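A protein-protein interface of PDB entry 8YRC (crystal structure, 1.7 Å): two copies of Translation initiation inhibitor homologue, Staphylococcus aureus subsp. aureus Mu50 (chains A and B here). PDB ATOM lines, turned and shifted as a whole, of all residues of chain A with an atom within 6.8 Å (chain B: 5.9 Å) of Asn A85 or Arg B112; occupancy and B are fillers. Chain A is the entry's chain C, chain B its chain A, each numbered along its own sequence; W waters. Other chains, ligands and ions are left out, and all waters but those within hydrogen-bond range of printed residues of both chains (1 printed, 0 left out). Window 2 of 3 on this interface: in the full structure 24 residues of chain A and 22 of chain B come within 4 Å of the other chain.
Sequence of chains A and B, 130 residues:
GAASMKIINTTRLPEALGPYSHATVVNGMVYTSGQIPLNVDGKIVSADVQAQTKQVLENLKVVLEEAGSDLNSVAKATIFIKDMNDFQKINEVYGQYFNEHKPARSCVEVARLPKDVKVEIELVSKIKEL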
ATOM      1  N   ILE A  81      19.089  23.925 -11.102  1.00  0.00           N
ATOM      2  CA  ILE A  81      18.014  24.508 -10.245  1.00  0.00           C
ATOM      3  C   ILE A  81      17.428  25.784 -10.856  1.00  0.00           C
ATOM      4  O   ILE A  81      18.041  26.483 -11.681  1.00  0.00           O
ATOM      5  CB  ILE A  81      18.522  24.736  -8.809  1.00  0.00           C
ATOM      6  CG1 ILE A  81      19.540  25.863  -8.663  1.00  0.00           C
ATOM      7  CG2 ILE A  81      19.056  23.449  -8.225  1.00  0.00           C
ATOM      8  CD1 ILE A  81      19.926  26.128  -7.219  1.00  0.00           C
ATOM      9  N   LYS A  82      16.214  26.093 -10.408  1.00  0.00           N
ATOM     10  CA  LYS A  82      15.482  27.287 -10.863  1.00  0.00           C
ATOM     11  C   LYS A  82      15.884  28.531 -10.067  1.00  0.00           C
ATOM     12  O   LYS A  82      15.800  29.619 -10.657  1.00  0.00           O
ATOM     13  CB  LYS A  82      13.982  27.057 -10.685  1.00  0.00           C
ATOM     14  CG  LYS A  82      13.105  28.199 -11.147  1.00  0.00           C
ATOM     15  CD  LYS A  82      13.436  28.548 -12.538  1.00  0.00           C
ATOM     16  CE  LYS A  82      12.521  29.628 -13.038  1.00  0.00           C
ATOM     17  NZ  LYS A  82      13.265  30.846 -13.369  1.00  0.00           N
ATOM     18  N   ASP A  83      16.322  28.354  -8.830  1.00  0.00           N
ATOM     19  CA  ASP A  83      16.568  29.480  -7.885  1.00  0.00           C
ATOM     20  C   ASP A  83      17.682  29.124  -6.908  1.00  0.00           C
ATOM     21  O   ASP A  83      17.467  28.416  -5.913  1.00  0.00           O
ATOM     22  CB  ASP A  83      15.267  29.874  -7.169  1.00  0.00           C
ATOM     23  CG  ASP A  83      15.370  31.210  -6.474  1.00  0.00           C
ATOM     24  OD1 ASP A  83      16.499  31.697  -6.278  1.00  0.00           O
ATOM     25  OD2 ASP A  83      14.313  31.762  -6.175  1.00  0.00           O
ATOM     26  N   MET A  84      18.829  29.773  -7.119  1.00  0.00           N
ATOM     27  CA  MET A  84      20.009  29.668  -6.221  1.00  0.00           C
ATOM     28  C   MET A  84      19.681  30.099  -4.780  1.00  0.00           C
ATOM     29  O   MET A  84      20.336  29.548  -3.864  1.00  0.00           O
ATOM     30  CB  MET A  84      21.198  30.435  -6.812  1.00  0.00           C
ATOM     31  CG  MET A  84      22.516  30.163  -6.132  1.00  0.00           C
ATOM     32  SD  MET A  84      23.140  28.467  -6.377  1.00  0.00           S
ATOM     33  CE  MET A  84      23.456  28.336  -8.138  1.00  0.00           C
ATOM     34  N   ASN A  85      18.695  30.958  -4.521  1.00  0.00           N
ATOM     35  CA  ASN A  85      18.240  31.240  -3.124  1.00  0.00           C
ATOM     36  C   ASN A  85      17.694  29.972  -2.449  1.00  0.00           C
ATOM     37  O   ASN A  85      17.770  29.865  -1.193  1.00  0.00           O
ATOM     38  CB  ASN A  85      17.284  32.427  -3.125  1.00  0.00           C
ATOM     39  CG  ASN A  85      17.951  33.717  -3.598  1.00  0.00           C
ATOM     40  OD1 ASN A  85      19.120  33.997  -3.335  1.00  0.00           O
ATOM     41  ND2 ASN A  85      17.204  34.508  -4.326  1.00  0.00           N
ATOM     42  N   ASP A  86      17.300  28.940  -3.213  1.00  0.00           N
ATOM     43  CA  ASP A  86      16.840  27.652  -2.636  1.00  0.00           C
ATOM     44  C   ASP A  86      18.002  26.691  -2.344  1.00  0.00           C
ATOM     45  O   ASP A  86      17.736  25.530  -1.924  1.00  0.00           O
ATOM     46  CB  ASP A  86      15.891  26.908  -3.593  1.00  0.00           C
ATOM     47  CG  ASP A  86      14.527  27.550  -3.794  1.00  0.00           C
ATOM     48  OD1 ASP A  86      14.102  28.302  -2.915  1.00  0.00           O
ATOM     49  OD2 ASP A  86      13.898  27.259  -4.849  1.00  0.00           O
ATOM     50  N   PHE A  87      19.239  27.069  -2.634  1.00  0.00           N
ATOM     51  CA  PHE A  87      20.413  26.166  -2.534  1.00  0.00           C
ATOM     52  C   PHE A  87      20.494  25.521  -1.149  1.00  0.00           C
ATOM     53  O   PHE A  87      20.711  24.314  -1.039  1.00  0.00           O
ATOM     54  CB  PHE A  87      21.710  26.886  -2.912  1.00  0.00           C
ATOM     55  CG  PHE A  87      22.863  25.941  -2.745  1.00  0.00           C
ATOM     56  CD1 PHE A  87      22.998  24.864  -3.612  1.00  0.00           C
ATOM     57  CD2 PHE A  87      23.648  25.986  -1.602  1.00  0.00           C
ATOM     58  CE1 PHE A  87      23.994  23.914  -3.416  1.00  0.00           C
ATOM     59  CE2 PHE A  87      24.661  25.062  -1.417  1.00  0.00           C
ATOM     60  CZ  PHE A  87      24.832  24.034  -2.323  1.00  0.00           C
ATOM     61  N   GLN A  88      20.380  26.302  -0.058  1.00  0.00           N
ATOM     62  CA  GLN A  88      20.521  25.674   1.286  1.00  0.00           C
ATOM     63  C   GLN A  88      19.427  24.602   1.486  1.00  0.00           C
ATOM     64  O   GLN A  88      19.760  23.571   2.099  1.00  0.00           O
ATOM     65  CB  GLN A  88      20.585  26.698   2.428  1.00  0.00           C
ATOM     66  CG  GLN A  88      21.979  27.288   2.708  1.00  0.00           C
ATOM     67  CD  GLN A  88      23.209  26.475   2.326  1.00  0.00           C
ATOM     68  OE1 GLN A  88      23.349  25.280   2.631  1.00  0.00           O
ATOM     69  NE2 GLN A  88      24.157  27.140   1.669  1.00  0.00           N
ATOM     70  N   LYS A  89      18.187  24.852   1.059  1.00  0.00           N
ATOM     71  CA  LYS A  89      17.052  23.922   1.271  1.00  0.00           C
ATOM     72  C   LYS A  89      17.297  22.657   0.444  1.00  0.00           C
ATOM     73  O   LYS A  89      17.112  21.524   0.969  1.00  0.00           O
ATOM     74  CB  LYS A  89      15.751  24.610   0.849  1.00  0.00           C
ATOM     75  CG  LYS A  89      15.098  25.444   1.933  1.00  0.00           C
ATOM     76  CD  LYS A  89      14.260  26.552   1.354  1.00  0.00           C
ATOM     77  CE  LYS A  89      13.291  27.142   2.361  1.00  0.00           C
ATOM     78  NZ  LYS A  89      12.334  28.049   1.686  1.00  0.00           N
ATOM     79  N   CYS A 107      26.461  22.584  -9.278  1.00  0.00           N
ATOM     80  CA  CYS A 107      25.115  23.119  -9.093  1.00  0.00           C
ATOM     81  C   CYS A 107      25.057  24.508  -9.742  1.00  0.00           C
ATOM     82  O   CYS A 107      25.847  25.368  -9.382  1.00  0.00           O
ATOM     83  CB  CYS A 107      24.747  23.094  -7.619  1.00  0.00           C
ATOM     84  SG  CYS A 107      23.098  23.766  -7.309  1.00  0.00           S
ATOM     85  N   VAL A 108      24.219  24.689 -10.741  1.00  0.00           N
ATOM     86  CA  VAL A 108      23.988  25.981 -11.448  1.00  0.00           C
ATOM     87  C   VAL A 108      22.469  26.259 -11.463  1.00  0.00           C
ATOM     88  O   VAL A 108      21.599  25.306 -11.554  1.00  0.00           O
ATOM     89  CB  VAL A 108      24.569  25.949 -12.877  1.00  0.00           C
ATOM     90  CG1 VAL A 108      26.063  25.657 -12.829  1.00  0.00           C
ATOM     91  CG2 VAL A 108      23.838  24.950 -13.766  1.00  0.00           C
ATOM     92  N   GLU A 109      22.160  27.535 -11.456  1.00  0.00           N
ATOM     93  CA  GLU A 109      20.802  28.030 -11.741  1.00  0.00           C
ATOM     94  C   GLU A 109      20.640  28.198 -13.238  1.00  0.00           C
ATOM     95  O   GLU A 109      21.343  29.039 -13.900  1.00  0.00           O
ATOM     96  CB  GLU A 109      20.529  29.342 -11.021  1.00  0.00           C
ATOM     97  CG  GLU A 109      19.075  29.778 -11.172  1.00  0.00           C
ATOM     98  CD  GLU A 109      18.787  31.137 -10.578  1.00  0.00           C
ATOM     99  OE1 GLU A 109      18.099  31.932 -11.275  1.00  0.00           O
ATOM    100  OE2 GLU A 109      19.071  31.298  -9.377  1.00  0.00           O
ATOM    101  N   VAL A 110      19.697  27.427 -13.790  1.00  0.00           N
ATOM    102  CA  VAL A 110      19.314  27.558 -15.215  1.00  0.00           C
ATOM    103  C   VAL A 110      18.146  28.559 -15.339  1.00  0.00           C
ATOM    104  O   VAL A 110      17.506  28.922 -14.308  1.00  0.00           O
ATOM    105  CB  VAL A 110      19.051  26.177 -15.847  1.00  0.00           C
ATOM    106  CG1 VAL A 110      20.341  25.360 -15.814  1.00  0.00           C
ATOM    107  CG2 VAL A 110      17.890  25.429 -15.201  1.00  0.00           C
ATOM    108  N   ALA A 111      17.806  28.885 -16.572  1.00  0.00           N
ATOM    109  CA  ALA A 111      16.677  29.789 -16.876  1.00  0.00           C
ATOM    110  C   ALA A 111      15.329  29.097 -16.592  1.00  0.00           C
ATOM    111  O   ALA A 111      14.425  29.784 -16.135  1.00  0.00           O
ATOM    112  CB  ALA A 111      16.797  30.308 -18.300  1.00  0.00           C
ATOM    113  N   LYS B  82      28.107  33.509 -16.537  1.00  0.00           N
ATOM    114  CA  LYS B  82      27.029  34.453 -16.181  1.00  0.00           C
ATOM    115  C   LYS B  82      26.703  35.313 -17.405  1.00  0.00           C
ATOM    116  O   LYS B  82      25.521  35.740 -17.514  1.00  0.00           O
ATOM    117  CB  LYS B  82      27.353  35.268 -14.919  1.00  0.00           C
ATOM    118  CG  LYS B  82      26.294  36.241 -14.499  1.00  0.00           C
ATOM    119  CD  LYS B  82      24.938  35.631 -14.185  1.00  0.00           C
ATOM    120  CE  LYS B  82      23.814  36.632 -14.220  1.00  0.00           C
ATOM    121  NZ  LYS B  82      23.597  37.157 -15.590  1.00  0.00           N
ATOM    122  N   VAL B 110      24.394  30.467 -18.010  1.00  0.00           N
ATOM    123  CA  VAL B 110      23.358  30.152 -17.000  1.00  0.00           C
ATOM    124  C   VAL B 110      22.686  31.397 -16.438  1.00  0.00           C
ATOM    125  O   VAL B 110      23.182  32.573 -16.708  1.00  0.00           O
ATOM    126  CB  VAL B 110      23.952  29.252 -15.884  1.00  0.00           C
ATOM    127  CG1 VAL B 110      24.460  27.964 -16.471  1.00  0.00           C
ATOM    128  CG2 VAL B 110      25.037  29.967 -15.108  1.00  0.00           C
ATOM    129  N   ALA B 111      21.645  31.210 -15.621  1.00  0.00           N
ATOM    130  CA  ALA B 111      20.934  32.336 -14.970  1.00  0.00           C
ATOM    131  C   ALA B 111      21.809  32.885 -13.833  1.00  0.00           C
ATOM    132  O   ALA B 111      21.881  34.130 -13.596  1.00  0.00           O
ATOM    133  CB  ALA B 111      19.586  31.876 -14.488  1.00  0.00           C
ATOM    134  N   ARG B 112      22.415  31.981 -13.079  1.00  0.00           N
ATOM    135  CA  ARG B 112      23.085  32.374 -11.808  1.00  0.00           C
ATOM    136  C   ARG B 112      24.040  31.253 -11.376  1.00  0.00           C
ATOM    137  O   ARG B 112      23.715  30.047 -11.571  1.00  0.00           O
ATOM    138  CB  ARG B 112      22.104  32.630 -10.664  1.00  0.00           C
ATOM    139  CG  ARG B 112      22.702  33.431  -9.518  1.00  0.00           C
ATOM    140  CD  ARG B 112      21.656  33.785  -8.489  1.00  0.00           C
ATOM    141  NE  ARG B 112      22.202  34.633  -7.443  1.00  0.00           N
ATOM    142  CZ  ARG B 112      21.661  34.796  -6.262  1.00  0.00           C
ATOM    143  NH1 ARG B 112      20.503  34.231  -5.959  1.00  0.00           N
ATOM    144  NH2 ARG B 112      22.261  35.551  -5.374  1.00  0.00           N
ATOM    145  N   LEU B 113      25.172  31.659 -10.811  1.00  0.00           N
ATOM    146  CA  LEU B 113      26.196  30.723 -10.291  1.00  0.00           C
ATOM    147  C   LEU B 113      26.324  30.915  -8.783  1.00  0.00           C
ATOM    148  O   LEU B 113      25.959  31.950  -8.221  1.00  0.00           O
ATOM    149  CB  LEU B 113      27.549  30.970 -10.960  1.00  0.00           C
ATOM    150  CG  LEU B 113      27.650  30.627 -12.455  1.00  0.00           C
ATOM    151  CD1 LEU B 113      29.004  31.048 -13.041  1.00  0.00           C
ATOM    152  CD2 LEU B 113      27.410  29.117 -12.657  1.00  0.00           C
ATOM    153  N   PRO B 114      26.890  29.921  -8.066  1.00  0.00           N
ATOM    154  CA  PRO B 114      27.067  30.017  -6.631  1.00  0.00           C
ATOM    155  C   PRO B 114      27.862  31.278  -6.299  1.00  0.00           C
ATOM    156  O   PRO B 114      28.831  31.629  -7.017  1.00  0.00           O
ATOM    157  CB  PRO B 114      27.868  28.795  -6.262  1.00  0.00           C
ATOM    158  CG  PRO B 114      27.405  27.780  -7.310  1.00  0.00           C
ATOM    159  CD  PRO B 114      27.321  28.601  -8.574  1.00  0.00           C
ATOM    160  N   ASP B 116      27.173  34.254  -6.865  1.00  0.00           N
ATOM    161  CA  ASP B 116      27.096  35.306  -7.904  1.00  0.00           C
ATOM    162  C   ASP B 116      28.438  35.431  -8.632  1.00  0.00           C
ATOM    163  O   ASP B 116      28.770  36.518  -9.160  1.00  0.00           O
ATOM    164  CB  ASP B 116      26.592  36.602  -7.265  1.00  0.00           C
ATOM    165  CG  ASP B 116      25.124  36.508  -6.962  1.00  0.00           C
ATOM    166  OD1 ASP B 116      24.365  36.407  -7.951  1.00  0.00           O
ATOM    167  OD2 ASP B 116      24.763  36.499  -5.763  1.00  0.00           O
ATOM    168  N   VAL B 117      29.234  34.369  -8.644  1.00  0.00           N
ATOM    169  CA  VAL B 117      30.438  34.343  -9.476  1.00  0.00           C
ATOM    170  C   VAL B 117      30.071  34.434 -10.967  1.00  0.00           C
ATOM    171  O   VAL B 117      28.910  34.156 -11.370  1.00  0.00           O
ATOM    172  CB  VAL B 117      31.347  33.133  -9.175  1.00  0.00           C
ATOM    173  CG1 VAL B 117      31.782  33.126  -7.725  1.00  0.00           C
ATOM    174  CG2 VAL B 117      30.742  31.824  -9.641  1.00  0.00           C
HETATM  175  O   HOH W   1      18.535  33.245  -7.585  1.00  0.00           O
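Among the printed residues, pairs that only touch across the chains: Glu A109 with Val B110, Cys A107 with Pro B114, Val A110 with Ala B111, Val A108 with Leu B113, Met A84 with Arg B112, Met A84 with Pro B114, Met A84 with Leu B113 and Val A108 with Arg B112.
Water W1 lies within hydrogen-bond range of OE2 of Glu A109, NH1 of Arg B112 and OD1 of Asp A83.
The backbone carbonyl oxygen (O) of Glu A109 is in hydrogen-bond range of the backbone NH (N) of Ala B111, at 2.8 Å. The guanidinium group of Arg B112 is in hydrogen-bond range of the side-chain amide oxygen of Asn A85. The backbone NH (N) of Glu A109 sits at hydrogen-bond distance from the backbone carbonyl oxygen (O) of Arg B112 (3.0 Å).
The side-chain carboxylate (OD2) of Asp B116 lies within salt-bridge range of the guanidinium group (NH2) of Arg B112, 2.7 Å away. The backbone carbonyl oxygen (O) of Val A108 is in hydrogen-bond range of the backbone NH (N) of Ile A81, 2.9 Å away. The backbone carbonyl oxygen (O) of Ile A81 sits at hydrogen-bond distance from the backbone NH (N) of Val A110. OD1 of Asp A83 lies within hydrogen-bond range of N of Asn A85, 2.9 Å away. The backbone NH of Met A84 sits at hydrogen-bond distance from the side-chain carboxylate of Glu A109.
Printed residues of chain B within 4 Å of Met A84: Arg B112 (3.8 Å), Leu B113 (3.9 Å) and Pro B114 (3.8 Å). Asn A85 touches just one residue of chain B: Arg B112 (3.0 Å). Of the printed residues of chain B, Val A108 touches Arg B112 and Leu B113. Ala A111 touches none of the printed residues of chain B. Printed residues of chain A within 4 Å of Val B110: Glu A109 (3.3 Å). Of the printed residues of chain A, Arg B112 touches Met A84, Asn A85, Val A108 and Glu A109. The nearest printed residue of chain B that does not touch Asn A85 is Asp B116 (6.6 Å).
Val A110 touches Ala B111, but with the chains exchanged Ala A111 does not touch Val B110 (5.5 Å). Of the 11 pairs that touch across the chains among the printed residues, none has its exchanged pair printed and touching as well.
Hydrophobic or aromatic side chains of chain A within 4 Å of the printed part of chain B: Met A84 and Val A108. Of the 8 printed residues of chain B, 5 touch a printed residue of chain A. Hydrophobic or aromatic side chains of chain B that line the printed part of chain A: Val B110, Ala B111, Leu B113 and Pro B114. Among the printed residues, no Asp or Glu carboxylate lies within 4 Å of a Lys or Arg side-chain nitrogen of the other chain.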
